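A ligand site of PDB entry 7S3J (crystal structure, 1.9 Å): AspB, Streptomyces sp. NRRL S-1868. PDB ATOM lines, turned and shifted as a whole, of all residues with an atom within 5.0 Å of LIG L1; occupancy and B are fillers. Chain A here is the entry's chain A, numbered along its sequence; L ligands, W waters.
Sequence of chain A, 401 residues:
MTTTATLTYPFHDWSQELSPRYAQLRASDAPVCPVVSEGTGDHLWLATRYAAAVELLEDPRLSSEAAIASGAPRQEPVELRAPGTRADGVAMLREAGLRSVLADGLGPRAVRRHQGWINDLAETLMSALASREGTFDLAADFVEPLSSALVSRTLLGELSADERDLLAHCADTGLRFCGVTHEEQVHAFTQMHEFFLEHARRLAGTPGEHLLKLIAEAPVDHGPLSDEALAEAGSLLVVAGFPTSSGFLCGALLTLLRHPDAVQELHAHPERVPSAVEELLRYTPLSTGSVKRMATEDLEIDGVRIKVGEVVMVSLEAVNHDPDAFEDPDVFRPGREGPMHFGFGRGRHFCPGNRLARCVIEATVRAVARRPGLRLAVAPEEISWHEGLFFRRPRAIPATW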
ATOM      1  N   SER A  64     -20.193 -29.033 -16.947  1.00  0.00           N
ATOM      2  CA  SER A  64     -21.258 -28.300 -17.624  1.00  0.00           C
ATOM      3  C   SER A  64     -21.925 -29.164 -18.688  1.00  0.00           C
ATOM      4  O   SER A  64     -23.147 -29.158 -18.840  1.00  0.00           O
ATOM      5  CB  SER A  64     -20.698 -27.014 -18.235  1.00  0.00           C
ATOM      6  OG  SER A  64     -21.612 -26.412 -19.137  1.00  0.00           O
ATOM      7  N   VAL A  90     -21.206 -25.365 -27.479  1.00  0.00           N
ATOM      8  CA  VAL A  90     -19.934 -25.089 -28.128  1.00  0.00           C
ATOM      9  C   VAL A  90     -19.062 -26.329 -28.243  1.00  0.00           C
ATOM     10  O   VAL A  90     -18.148 -26.354 -29.084  1.00  0.00           O
ATOM     11  CB  VAL A  90     -19.167 -23.989 -27.367  1.00  0.00           C
ATOM     12  CG1 VAL A  90     -20.077 -22.840 -27.045  1.00  0.00           C
ATOM     13  CG2 VAL A  90     -18.577 -24.557 -26.086  1.00  0.00           C
ATOM     14  N   LEU A 106     -14.327 -14.289 -32.100  1.00  0.00           N
ATOM     15  CA  LEU A 106     -14.716 -13.605 -30.869  1.00  0.00           C
ATOM     16  C   LEU A 106     -13.529 -12.999 -30.116  1.00  0.00           C
ATOM     17  O   LEU A 106     -13.734 -12.333 -29.099  1.00  0.00           O
ATOM     18  CB  LEU A 106     -15.488 -14.569 -29.954  1.00  0.00           C
ATOM     19  CG  LEU A 106     -16.676 -15.346 -30.562  1.00  0.00           C
ATOM     20  CD1 LEU A 106     -17.127 -16.450 -29.630  1.00  0.00           C
ATOM     21  CD2 LEU A 106     -17.872 -14.413 -30.875  1.00  0.00           C
ATOM     22  N   LEU A 150     -24.881  -5.999 -33.876  1.00  0.00           N
ATOM     23  CA  LEU A 150     -23.918  -6.925 -33.259  1.00  0.00           C
ATOM     24  C   LEU A 150     -24.123  -8.360 -33.712  1.00  0.00           C
ATOM     25  O   LEU A 150     -23.227  -8.960 -34.324  1.00  0.00           O
ATOM     26  CB  LEU A 150     -24.007  -6.804 -31.739  1.00  0.00           C
ATOM     27  CG  LEU A 150     -23.136  -7.850 -31.058  1.00  0.00           C
ATOM     28  CD1 LEU A 150     -21.821  -7.293 -30.627  1.00  0.00           C
ATOM     29  CD2 LEU A 150     -23.910  -8.316 -29.844  1.00  0.00           C
ATOM     30  N   LEU A 155     -21.840 -12.266 -35.853  1.00  0.00           N
ATOM     31  CA  LEU A 155     -22.161 -13.694 -35.737  1.00  0.00           C
ATOM     32  C   LEU A 155     -22.827 -14.292 -36.963  1.00  0.00           C
ATOM     33  O   LEU A 155     -22.371 -15.319 -37.477  1.00  0.00           O
ATOM     34  CB  LEU A 155     -23.054 -13.950 -34.524  1.00  0.00           C
ATOM     35  CG  LEU A 155     -22.593 -13.436 -33.157  1.00  0.00           C
ATOM     36  CD1 LEU A 155     -23.530 -13.963 -32.065  1.00  0.00           C
ATOM     37  CD2 LEU A 155     -21.129 -13.837 -32.879  1.00  0.00           C
ATOM     38  N   LEU A 236     -27.007 -22.001 -31.678  1.00  0.00           N
ATOM     39  CA  LEU A 236     -26.171 -21.636 -30.536  1.00  0.00           C
ATOM     40  C   LEU A 236     -25.809 -20.146 -30.528  1.00  0.00           C
ATOM     41  O   LEU A 236     -25.894 -19.476 -29.481  1.00  0.00           O
ATOM     42  CB  LEU A 236     -24.912 -22.501 -30.553  1.00  0.00           C
ATOM     43  CG  LEU A 236     -23.779 -22.085 -29.621  1.00  0.00           C
ATOM     44  CD1 LEU A 236     -24.046 -22.621 -28.212  1.00  0.00           C
ATOM     45  CD2 LEU A 236     -22.436 -22.580 -30.170  1.00  0.00           C
ATOM     46  N   ALA A 240     -26.931 -17.804 -27.479  1.00  0.00           N
ATOM     47  CA  ALA A 240     -25.911 -17.278 -26.582  1.00  0.00           C
ATOM     48  C   ALA A 240     -25.785 -15.769 -26.672  1.00  0.00           C
ATOM     49  O   ALA A 240     -25.426 -15.129 -25.673  1.00  0.00           O
ATOM     50  CB  ALA A 240     -24.553 -17.930 -26.866  1.00  0.00           C
ATOM     51  N   GLY A 241     -26.076 -15.173 -27.826  1.00  0.00           N
ATOM     52  CA  GLY A 241     -25.663 -13.805 -28.077  1.00  0.00           C
ATOM     53  C   GLY A 241     -26.761 -12.760 -28.089  1.00  0.00           C
ATOM     54  O   GLY A 241     -26.537 -11.640 -27.604  1.00  0.00           O
ATOM     55  N   THR A 244     -29.199 -12.345 -24.438  1.00  0.00           N
ATOM     56  CA  THR A 244     -28.250 -11.889 -23.432  1.00  0.00           C
ATOM     57  C   THR A 244     -27.837 -10.436 -23.697  1.00  0.00           C
ATOM     58  O   THR A 244     -27.911  -9.582 -22.811  1.00  0.00           O
ATOM     59  CB  THR A 244     -27.033 -12.806 -23.474  1.00  0.00           C
ATOM     60  OG1 THR A 244     -26.650 -12.949 -24.850  1.00  0.00           O
ATOM     61  CG2 THR A 244     -27.400 -14.199 -22.932  1.00  0.00           C
ATOM     62  N   SER A 245     -27.403 -10.144 -24.928  1.00  0.00           N
ATOM     63  CA  SER A 245     -26.931  -8.795 -25.240  1.00  0.00           C
ATOM     64  C   SER A 245     -28.058  -7.760 -25.146  1.00  0.00           C
ATOM     65  O   SER A 245     -27.856  -6.654 -24.622  1.00  0.00           O
ATOM     66  CB  SER A 245     -26.324  -8.768 -26.651  1.00  0.00           C
ATOM     67  OG  SER A 245     -25.215  -9.662 -26.759  1.00  0.00           O
ATOM     68  N   PHE A 248     -29.115  -7.400 -21.347  1.00  0.00           N
ATOM     69  CA  PHE A 248     -28.145  -6.634 -20.571  1.00  0.00           C
ATOM     70  C   PHE A 248     -28.105  -5.169 -20.964  1.00  0.00           C
ATOM     71  O   PHE A 248     -28.070  -4.292 -20.095  1.00  0.00           O
ATOM     72  CB  PHE A 248     -26.746  -7.228 -20.718  1.00  0.00           C
ATOM     73  CG  PHE A 248     -25.751  -6.612 -19.783  1.00  0.00           C
ATOM     74  CD1 PHE A 248     -25.668  -7.035 -18.484  1.00  0.00           C
ATOM     75  CD2 PHE A 248     -24.957  -5.564 -20.196  1.00  0.00           C
ATOM     76  CE1 PHE A 248     -24.765  -6.448 -17.607  1.00  0.00           C
ATOM     77  CE2 PHE A 248     -24.072  -4.976 -19.334  1.00  0.00           C
ATOM     78  CZ  PHE A 248     -23.978  -5.402 -18.042  1.00  0.00           C
ATOM     79  N   LEU A 281     -21.508  -4.689 -15.391  1.00  0.00           N
ATOM     80  CA  LEU A 281     -21.585  -6.148 -15.461  1.00  0.00           C
ATOM     81  C   LEU A 281     -21.795  -6.783 -14.091  1.00  0.00           C
ATOM     82  O   LEU A 281     -22.405  -7.855 -13.983  1.00  0.00           O
ATOM     83  CB  LEU A 281     -20.334  -6.707 -16.129  1.00  0.00           C
ATOM     84  CG  LEU A 281     -20.366  -6.444 -17.631  1.00  0.00           C
ATOM     85  CD1 LEU A 281     -18.963  -6.302 -18.206  1.00  0.00           C
ATOM     86  CD2 LEU A 281     -21.171  -7.528 -18.338  1.00  0.00           C
ATOM     87  N   LEU A 286     -28.953  -9.931 -14.821  1.00  0.00           N
ATOM     88  CA  LEU A 286     -29.415 -10.413 -16.113  1.00  0.00           C
ATOM     89  C   LEU A 286     -30.251 -11.697 -16.003  1.00  0.00           C
ATOM     90  O   LEU A 286     -31.427 -11.683 -16.326  1.00  0.00           O
ATOM     91  CB  LEU A 286     -28.217 -10.619 -17.025  1.00  0.00           C
ATOM     92  CG  LEU A 286     -28.585 -11.127 -18.414  1.00  0.00           C
ATOM     93  CD1 LEU A 286     -29.628 -10.154 -19.118  1.00  0.00           C
ATOM     94  CD2 LEU A 286     -27.323 -11.347 -19.238  1.00  0.00           C
ATOM     95  N   VAL A 291     -26.175 -20.407 -13.494  1.00  0.00           N
ATOM     96  CA  VAL A 291     -25.270 -21.335 -14.174  1.00  0.00           C
ATOM     97  C   VAL A 291     -25.246 -22.637 -13.386  1.00  0.00           C
ATOM     98  O   VAL A 291     -25.521 -22.654 -12.180  1.00  0.00           O
ATOM     99  CB  VAL A 291     -23.855 -20.735 -14.321  1.00  0.00           C
ATOM    100  CG1 VAL A 291     -23.946 -19.331 -14.865  1.00  0.00           C
ATOM    101  CG2 VAL A 291     -23.128 -20.755 -12.990  1.00  0.00           C
ATOM    102  N   LYS A 292     -24.968 -23.742 -14.050  1.00  0.00           N
ATOM    103  CA  LYS A 292     -25.208 -25.018 -13.403  1.00  0.00           C
ATOM    104  C   LYS A 292     -24.217 -26.062 -13.875  1.00  0.00           C
ATOM    105  O   LYS A 292     -23.775 -26.039 -15.032  1.00  0.00           O
ATOM    106  CB  LYS A 292     -26.674 -25.511 -13.604  1.00  0.00           C
ATOM    107  CG  LYS A 292     -26.962 -26.234 -14.916  1.00  0.00           C
ATOM    108  CD  LYS A 292     -26.966 -25.261 -16.095  1.00  0.00           C
ATOM    109  CE  LYS A 292     -27.536 -25.909 -17.300  1.00  0.00           C
ATOM    110  NZ  LYS A 292     -27.017 -25.314 -18.559  1.00  0.00           N
ATOM    111  N   ARG A 293     -23.867 -26.996 -12.973  1.00  0.00           N
ATOM    112  CA  ARG A 293     -22.858 -28.020 -13.233  1.00  0.00           C
ATOM    113  C   ARG A 293     -23.243 -29.323 -12.513  1.00  0.00           C
ATOM    114  O   ARG A 293     -23.845 -29.307 -11.428  1.00  0.00           O
ATOM    115  CB  ARG A 293     -21.461 -27.590 -12.752  1.00  0.00           C
ATOM    116  CG  ARG A 293     -21.009 -26.178 -13.150  1.00  0.00           C
ATOM    117  CD  ARG A 293     -20.252 -26.206 -14.458  1.00  0.00           C
ATOM    118  NE  ARG A 293     -19.729 -24.892 -14.835  1.00  0.00           N
ATOM    119  CZ  ARG A 293     -20.368 -24.017 -15.601  1.00  0.00           C
ATOM    120  NH1 ARG A 293     -21.606 -24.229 -16.027  1.00  0.00           N
ATOM    121  NH2 ARG A 293     -19.740 -22.888 -15.972  1.00  0.00           N
ATOM    122  N   LEU A 316     -25.246 -15.961 -10.616  1.00  0.00           N
ATOM    123  CA  LEU A 316     -24.311 -14.844 -10.788  1.00  0.00           C
ATOM    124  C   LEU A 316     -24.834 -13.559 -10.141  1.00  0.00           C
ATOM    125  O   LEU A 316     -24.047 -12.755  -9.615  1.00  0.00           O
ATOM    126  CB  LEU A 316     -24.059 -14.612 -12.259  1.00  0.00           C
ATOM    127  CG  LEU A 316     -23.722 -15.923 -12.947  1.00  0.00           C
ATOM    128  CD1 LEU A 316     -23.635 -15.666 -14.414  1.00  0.00           C
ATOM    129  CD2 LEU A 316     -22.387 -16.459 -12.406  1.00  0.00           C
ATOM    130  N   PHE A 342     -18.778 -11.683 -11.526  1.00  0.00           N
ATOM    131  CA  PHE A 342     -19.225 -12.925 -12.153  1.00  0.00           C
ATOM    132  C   PHE A 342     -20.219 -12.692 -13.301  1.00  0.00           C
ATOM    133  O   PHE A 342     -21.116 -13.520 -13.495  1.00  0.00           O
ATOM    134  CB  PHE A 342     -19.841 -13.845 -11.121  1.00  0.00           C
ATOM    135  CG  PHE A 342     -18.841 -14.677 -10.387  1.00  0.00           C
ATOM    136  CD1 PHE A 342     -17.983 -14.087  -9.461  1.00  0.00           C
ATOM    137  CD2 PHE A 342     -18.754 -16.030 -10.616  1.00  0.00           C
ATOM    138  CE1 PHE A 342     -17.056 -14.859  -8.774  1.00  0.00           C
ATOM    139  CE2 PHE A 342     -17.817 -16.797  -9.942  1.00  0.00           C
ATOM    140  CZ  PHE A 342     -16.969 -16.209  -9.017  1.00  0.00           C
ATOM    141  N   GLY A 343     -20.068 -11.596 -14.047  1.00  0.00           N
ATOM    142  CA  GLY A 343     -21.027 -11.256 -15.076  1.00  0.00           C
ATOM    143  C   GLY A 343     -20.910 -12.084 -16.341  1.00  0.00           C
ATOM    144  O   GLY A 343     -21.921 -12.285 -17.037  1.00  0.00           O
ATOM    145  N   PHE A 344     -19.721 -12.575 -16.663  1.00  0.00           N
ATOM    146  CA  PHE A 344     -19.494 -13.502 -17.773  1.00  0.00           C
ATOM    147  C   PHE A 344     -19.123 -14.911 -17.295  1.00  0.00           C
ATOM    148  O   PHE A 344     -18.571 -15.708 -18.063  1.00  0.00           O
ATOM    149  CB  PHE A 344     -18.357 -13.007 -18.685  1.00  0.00           C
ATOM    150  CG  PHE A 344     -18.630 -11.713 -19.395  1.00  0.00           C
ATOM    151  CD1 PHE A 344     -19.744 -11.574 -20.231  1.00  0.00           C
ATOM    152  CD2 PHE A 344     -17.738 -10.646 -19.267  1.00  0.00           C
ATOM    153  CE1 PHE A 344     -19.975 -10.382 -20.922  1.00  0.00           C
ATOM    154  CE2 PHE A 344     -17.961  -9.447 -19.949  1.00  0.00           C
ATOM    155  CZ  PHE A 344     -19.076  -9.304 -20.776  1.00  0.00           C
ATOM    156  N   GLY A 345     -19.357 -15.213 -16.026  1.00  0.00           N
ATOM    157  CA  GLY A 345     -18.958 -16.493 -15.489  1.00  0.00           C
ATOM    158  C   GLY A 345     -17.518 -16.485 -14.982  1.00  0.00           C
ATOM    159  O   GLY A 345     -16.899 -15.435 -14.729  1.00  0.00           O
ATOM    160  N   ARG A 348     -13.525 -22.448 -16.737  1.00  0.00           N
ATOM    161  CA  ARG A 348     -13.416 -22.985 -18.099  1.00  0.00           C
ATOM    162  C   ARG A 348     -14.499 -22.457 -19.046  1.00  0.00           C
ATOM    163  O   ARG A 348     -14.235 -22.342 -20.263  1.00  0.00           O
ATOM    164  CB  ARG A 348     -13.496 -24.505 -18.054  1.00  0.00           C
ATOM    165  CG  ARG A 348     -13.282 -25.163 -19.398  1.00  0.00           C
ATOM    166  CD  ARG A 348     -12.717 -26.570 -19.261  1.00  0.00           C
ATOM    167  NE  ARG A 348     -13.119 -27.395 -20.395  1.00  0.00           N
ATOM    168  CZ  ARG A 348     -13.693 -28.589 -20.281  1.00  0.00           C
ATOM    169  NH1 ARG A 348     -13.862 -29.167 -19.099  1.00  0.00           N
ATOM    170  NH2 ARG A 348     -14.115 -29.211 -21.382  1.00  0.00           N
ATOM    171  N   HIS A 349     -15.702 -22.141 -18.546  1.00  0.00           N
ATOM    172  CA  HIS A 349     -16.803 -21.751 -19.429  1.00  0.00           C
ATOM    173  C   HIS A 349     -17.103 -20.243 -19.405  1.00  0.00           C
ATOM    174  O   HIS A 349     -18.193 -19.825 -19.803  1.00  0.00           O
ATOM    175  CB  HIS A 349     -18.067 -22.555 -19.095  1.00  0.00           C
ATOM    176  CG  HIS A 349     -17.853 -24.027 -19.224  1.00  0.00           C
ATOM    177  ND1 HIS A 349     -17.667 -24.632 -20.453  1.00  0.00           N
ATOM    178  CD2 HIS A 349     -17.724 -24.996 -18.294  1.00  0.00           C
ATOM    179  CE1 HIS A 349     -17.436 -25.919 -20.266  1.00  0.00           C
ATOM    180  NE2 HIS A 349     -17.486 -26.169 -18.971  1.00  0.00           N
ATOM    181  N   PHE A 350     -16.147 -19.436 -18.956  1.00  0.00           N
ATOM    182  CA  PHE A 350     -16.147 -17.993 -19.123  1.00  0.00           C
ATOM    183  C   PHE A 350     -16.673 -17.612 -20.497  1.00  0.00           C
ATOM    184  O   PHE A 350     -16.287 -18.197 -21.517  1.00  0.00           O
ATOM    185  CB  PHE A 350     -14.686 -17.507 -18.954  1.00  0.00           C
ATOM    186  CG  PHE A 350     -14.545 -16.016 -18.857  1.00  0.00           C
ATOM    187  CD1 PHE A 350     -15.015 -15.327 -17.746  1.00  0.00           C
ATOM    188  CD2 PHE A 350     -13.924 -15.303 -19.864  1.00  0.00           C
ATOM    189  CE1 PHE A 350     -14.879 -13.946 -17.658  1.00  0.00           C
ATOM    190  CE2 PHE A 350     -13.777 -13.925 -19.784  1.00  0.00           C
ATOM    191  CZ  PHE A 350     -14.255 -13.242 -18.683  1.00  0.00           C
ATOM    192  N   CYS A 351     -17.596 -16.645 -20.527  1.00  0.00           N
ATOM    193  CA  CYS A 351     -18.227 -16.243 -21.791  1.00  0.00           C
ATOM    194  C   CYS A 351     -17.187 -15.969 -22.873  1.00  0.00           C
ATOM    195  O   CYS A 351     -16.357 -15.070 -22.708  1.00  0.00           O
ATOM    196  CB  CYS A 351     -19.077 -14.991 -21.598  1.00  0.00           C
ATOM    197  SG  CYS A 351     -19.740 -14.317 -23.208  1.00  0.00           S
ATOM    198  N   PRO A 352     -17.186 -16.729 -23.965  1.00  0.00           N
ATOM    199  CA  PRO A 352     -16.290 -16.408 -25.087  1.00  0.00           C
ATOM    200  C   PRO A 352     -16.750 -15.218 -25.931  1.00  0.00           C
ATOM    201  O   PRO A 352     -15.941 -14.702 -26.726  1.00  0.00           O
ATOM    202  CB  PRO A 352     -16.287 -17.688 -25.918  1.00  0.00           C
ATOM    203  CG  PRO A 352     -17.590 -18.349 -25.590  1.00  0.00           C
ATOM    204  CD  PRO A 352     -18.009 -17.922 -24.218  1.00  0.00           C
ATOM    205  N   GLY A 353     -17.994 -14.778 -25.810  1.00  0.00           N
ATOM    206  CA  GLY A 353     -18.392 -13.533 -26.409  1.00  0.00           C
ATOM    207  C   GLY A 353     -18.075 -12.311 -25.560  1.00  0.00           C
ATOM    208  O   GLY A 353     -18.574 -11.222 -25.855  1.00  0.00           O
ATOM    209  N   LEU A 356     -16.649  -9.006 -27.295  1.00  0.00           N
ATOM    210  CA  LEU A 356     -17.675  -8.325 -28.087  1.00  0.00           C
ATOM    211  C   LEU A 356     -18.708  -7.661 -27.186  1.00  0.00           C
ATOM    212  O   LEU A 356     -19.072  -6.496 -27.407  1.00  0.00           O
ATOM    213  CB  LEU A 356     -18.358  -9.313 -29.025  1.00  0.00           C
ATOM    214  CG  LEU A 356     -17.480  -9.777 -30.159  1.00  0.00           C
ATOM    215  CD1 LEU A 356     -18.237 -10.784 -31.041  1.00  0.00           C
ATOM    216  CD2 LEU A 356     -16.952  -8.587 -30.952  1.00  0.00           C
ATOM    217  N   ALA A 357     -19.187  -8.384 -26.172  1.00  0.00           N
ATOM    218  CA  ALA A 357     -20.153  -7.787 -25.256  1.00  0.00           C
ATOM    219  C   ALA A 357     -19.588  -6.521 -24.623  1.00  0.00           C
ATOM    220  O   ALA A 357     -20.241  -5.465 -24.635  1.00  0.00           O
ATOM    221  CB  ALA A 357     -20.558  -8.804 -24.180  1.00  0.00           C
HETATM  222  C1  LIG L   1     -21.438 -18.354 -21.882  1.00  0.00           C
HETATM  223  C2  LIG L   1     -21.525 -16.506 -26.358  1.00  0.00           C
HETATM  224  C3  LIG L   1     -22.972 -12.323 -24.546  1.00  0.00           C
HETATM  225  C4  LIG L   1     -22.623 -14.028 -20.037  1.00  0.00           C
HETATM  226  C5  LIG L   1     -21.432 -18.246 -23.255  1.00  0.00           C
HETATM  227  C6  LIG L   1     -21.290 -19.349 -24.198  1.00  0.00           C
HETATM  228  C7  LIG L   1     -21.302 -18.814 -25.432  1.00  0.00           C
HETATM  229  C8  LIG L   1     -21.470 -17.386 -25.305  1.00  0.00           C
HETATM  230  C9  LIG L   1     -21.201 -19.519 -26.804  1.00  0.00           C
HETATM  231  C10 LIG L   1     -21.137 -20.865 -23.836  1.00  0.00           C
HETATM  232  C11 LIG L   1     -19.826 -21.121 -23.109  1.00  0.00           C
HETATM  233  C12 LIG L   1     -19.716 -22.549 -22.630  1.00  0.00           C
HETATM  234  O1  LIG L   1     -18.558 -23.017 -22.448  1.00  0.00           O
HETATM  235  O2  LIG L   1     -20.768 -23.233 -22.455  1.00  0.00           O
HETATM  236  C13 LIG L   1     -21.869 -15.192 -26.243  1.00  0.00           C
HETATM  237  C14 LIG L   1     -21.917 -14.255 -27.339  1.00  0.00           C
HETATM  238  C15 LIG L   1     -22.332 -13.082 -26.820  1.00  0.00           C
HETATM  239  C16 LIG L   1     -22.523 -13.274 -25.407  1.00  0.00           C
HETATM  240  C17 LIG L   1     -21.542 -14.678 -28.779  1.00  0.00           C
HETATM  241  C18 LIG L   1     -22.540 -11.700 -27.486  1.00  0.00           C
HETATM  242  C19 LIG L   1     -22.059 -11.400 -28.690  1.00  0.00           C
HETATM  243  C20 LIG L   1     -23.034 -12.449 -23.196  1.00  0.00           C
HETATM  244  C21 LIG L   1     -23.421 -11.359 -22.323  1.00  0.00           C
HETATM  245  C22 LIG L   1     -23.328 -11.837 -21.060  1.00  0.00           C
HETATM  246  C23 LIG L   1     -22.869 -13.215 -21.120  1.00  0.00           C
HETATM  247  C24 LIG L   1     -23.869  -9.961 -22.830  1.00  0.00           C
HETATM  248  C25 LIG L   1     -23.611 -11.115 -19.717  1.00  0.00           C
HETATM  249  C26 LIG L   1     -23.948  -9.825 -19.645  1.00  0.00           C
HETATM  250  C27 LIG L   1     -22.268 -15.350 -20.146  1.00  0.00           C
HETATM  251  C28 LIG L   1     -22.111 -16.269 -19.053  1.00  0.00           C
HETATM  252  C29 LIG L   1     -21.789 -17.460 -19.532  1.00  0.00           C
HETATM  253  C30 LIG L   1     -21.734 -17.360 -20.985  1.00  0.00           C
HETATM  254  C31 LIG L   1     -22.314 -15.872 -17.581  1.00  0.00           C
HETATM  255  C32 LIG L   1     -21.467 -18.710 -18.653  1.00  0.00           C
HETATM  256  C33 LIG L   1     -22.352 -19.938 -18.839  1.00  0.00           C
HETATM  257  C34 LIG L   1     -21.982 -20.982 -17.791  1.00  0.00           C
HETATM  258  O3  LIG L   1     -20.999 -20.763 -17.040  1.00  0.00           O
HETATM  259  O4  LIG L   1     -22.654 -22.048 -17.684  1.00  0.00           O
HETATM  260  N1  LIG L   1     -21.548 -17.055 -23.984  1.00  0.00           N
HETATM  261  N2  LIG L   1     -22.255 -14.566 -25.072  1.00  0.00           N
HETATM  262  N3  LIG L   1     -22.707 -13.571 -22.436  1.00  0.00           N
HETATM  263  N4  LIG L   1     -22.034 -16.050 -21.325  1.00  0.00           N
HETATM  264 FE1  LIG L   1     -21.917 -15.239 -23.239  1.00  0.00          FE
HETATM  265  C1  LG2 L   2     -25.742 -23.912 -21.623  1.00  0.00           C
HETATM  266  N1  LG2 L   2     -23.507 -23.157 -22.509  1.00  0.00           N
HETATM  267  O1  LG2 L   2     -26.435 -24.204 -20.657  1.00  0.00           O
HETATM  268  C2  LG2 L   2     -24.417 -23.234 -21.365  1.00  0.00           C
HETATM  269  C3  LG2 L   2     -24.673 -21.844 -20.790  1.00  0.00           C
HETATM  270  C4  LG2 L   2     -25.328 -20.853 -21.753  1.00  0.00           C
HETATM  271  O2  LG2 L   2     -22.930 -23.638 -24.613  1.00  0.00           O
HETATM  272  C5  LG2 L   2     -27.493 -23.386 -24.587  1.00  0.00           C
HETATM  273  C6  LG2 L   2     -26.032 -23.085 -24.917  1.00  0.00           C
HETATM  274  C7  LG2 L   2     -27.493 -24.340 -23.396  1.00  0.00           C
HETATM  275  C8  LG2 L   2     -23.801 -23.587 -23.733  1.00  0.00           C
HETATM  276  C9  LG2 L   2     -25.223 -24.040 -24.030  1.00  0.00           C
HETATM  277  N2  LG2 L   2     -26.142 -24.118 -22.887  1.00  0.00           N
HETATM  278  C10 LG2 L   2     -24.667 -19.873 -22.486  1.00  0.00           C
HETATM  279  C11 LG2 L   2     -26.689 -20.688 -22.053  1.00  0.00           C
HETATM  280  N3  LG2 L   2     -25.581 -19.161 -23.218  1.00  0.00           N
HETATM  281  C12 LG2 L   2     -26.810 -19.636 -22.959  1.00  0.00           C
HETATM  282  C13 LG2 L   2     -27.817 -21.387 -21.592  1.00  0.00           C
HETATM  283  C14 LG2 L   2     -29.215 -19.985 -22.971  1.00  0.00           C
HETATM  284  C15 LG2 L   2     -28.089 -19.286 -23.409  1.00  0.00           C
HETATM  285  C16 LG2 L   2     -29.075 -21.030 -22.054  1.00  0.00           C
HETATM  286  C1  LG3 L   3     -28.263 -21.407 -17.951  1.00  0.00           C
HETATM  287  N1  LG3 L   3     -29.037 -19.128 -17.514  1.00  0.00           N
HETATM  288  O1  LG3 L   3     -27.350 -22.211 -17.817  1.00  0.00           O
HETATM  289  C2  LG3 L   3     -27.933 -19.946 -17.990  1.00  0.00           C
HETATM  290  C3  LG3 L   3     -26.590 -19.675 -17.255  1.00  0.00           C
HETATM  291  C4  LG3 L   3     -26.400 -18.177 -17.153  1.00  0.00           C
HETATM  292  O2  LG3 L   3     -31.257 -18.816 -17.288  1.00  0.00           O
HETATM  293  C5  LG3 L   3     -31.642 -22.845 -17.836  1.00  0.00           C
HETATM  294  C6  LG3 L   3     -31.830 -21.341 -17.814  1.00  0.00           C
HETATM  295  C7  LG3 L   3     -30.126 -23.102 -17.876  1.00  0.00           C
HETATM  296  C8  LG3 L   3     -30.311 -19.475 -17.707  1.00  0.00           C
HETATM  297  C9  LG3 L   3     -30.582 -20.754 -18.423  1.00  0.00           C
HETATM  298  N2  LG3 L   3     -29.552 -21.760 -18.073  1.00  0.00           N
HETATM  299  C10 LG3 L   3     -26.499 -17.395 -16.010  1.00  0.00           C
HETATM  300  C11 LG3 L   3     -26.131 -17.302 -18.196  1.00  0.00           C
HETATM  301  N3  LG3 L   3     -26.291 -16.091 -16.365  1.00  0.00           N
HETATM  302  C12 LG3 L   3     -26.062 -16.020 -17.691  1.00  0.00           C
HETATM  303  C13 LG3 L   3     -25.958 -17.568 -19.538  1.00  0.00           C
HETATM  304  C14 LG3 L   3     -25.611 -15.218 -19.904  1.00  0.00           C
HETATM  305  C15 LG3 L   3     -25.805 -14.949 -18.555  1.00  0.00           C
HETATM  306  C16 LG3 L   3     -25.680 -16.512 -20.390  1.00  0.00           C
HETATM  307  O   HOH W   1     -24.185 -16.630 -23.788  1.00  0.00           O
HETATM  308  O   HOH W   2     -24.804 -23.014 -16.874  1.00  0.00           O
HETATM  309  O   HOH W   3     -16.344 -22.438 -23.934  1.00  0.00           O
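An iron atom (FE1) of LIG L1 is bound by the side-chain sulfur (SG) of Cys 351 (2.4 Å).
The guanidinium group (NH2) of Arg 293 lies within salt-bridge range of an oxygen (O3) of LIG L1.
O1 of LIG L1 lies within hydrogen-bond range of ND1 of His 349, at 2.7 Å.
An oxygen (O1) of LG2 L2 is in hydrogen-bond range of the side-chain amino group (NZ) of Lys 292.
O1 of LG3 L3 sits at hydrogen-bond distance from NZ of Lys 292 (3.2 Å).
N1 of LG2 L2 is in hydrogen-bond range of O2 of LIG L1.
The backbone NH of Cys 351 sits at hydrogen-bond distance from the backbone carbonyl oxygen of Phe 344, 2.8 Å away.
The side-chain sulfur (SG) of Cys 351 lies close to the backbone NH (N) of Gly 353 (3.2 Å).
The side-chain hydroxyl of Thr 244 is in hydrogen-bond range of the backbone carbonyl oxygen of Ala 240, 2.6 Å away.
O of Gly 241 sits at hydrogen-bond distance from OG of Ser 245.
OG1 of Thr 244 is in hydrogen-bond range of O of Gly 241 (3.1 Å).
The backbone carbonyl oxygen (O) of Ala 240 lies close to a nitrogen (N2) of LIG L1 (3.3 Å).
Val 90 touches LIG L1.
Leu 150 touches LIG L1.
Leu 155 touches LIG L1 (CD1 to C17, 3.9 Å).
Gly 241 touches LIG L1.
Thr 244 touches LIG L1.
Ser 245 touches LIG L1.
Phe 248 touches LIG L1 (CD1 to C26, 3.5 Å).
CD2 of Leu 281 touches C26 of LIG L1, at 3.8 Å.
CD2 of Leu 286 touches C26 of LIG L1 (3.7 Å).
Val 291 touches LIG L1 (CB to O4, 3.8 Å).
Leu 316 touches LIG L1.
Gly 343 touches LIG L1 (O to C25, 3.4 Å).
C of Phe 344 touches C31 of LIG L1, at 3.3 Å.
Gly 345 touches LIG L1.
CD of Pro 352 touches C5 of LIG L1, at 3.6 Å.
CA of Gly 353 touches C14 of LIG L1, at 3.7 Å.
Ala 357 touches LIG L1.
Hydrophobic or aromatic side chains within 4 Å of LIG L1: Val 90, Leu 150, Leu 155, Ala 240, Phe 248, Leu 281, Leu 286, Val 291, Leu 316, Phe 344, His 349, Pro 352 and Ala 357.
Within 4 Å of LIG L1: Val 90, Leu 150, Leu 155, Ala 240, Gly 241, Thr 244, Ser 245, Phe 248, Leu 281, Leu 286, Val 291, Arg 293, Leu 316, Gly 343, Phe 344, Gly 345, His 349, Cys 351, Pro 352, Gly 353 and Ala 357.
The nearest printed residue that does not touch LIG L1 is Leu 106 (4.2 Å).
Water W2 lies within hydrogen-bond range of an oxygen (O4) of LIG L1 (2.5 Å), an oxygen (O1) of LG3 L3 (2.8 Å) and the backbone NH of Lys 292 (2.9 Å).
Water W1 lies within hydrogen-bond range of the backbone carbonyl oxygen of Ala 240 and a nitrogen (N3) of LG2 L2.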
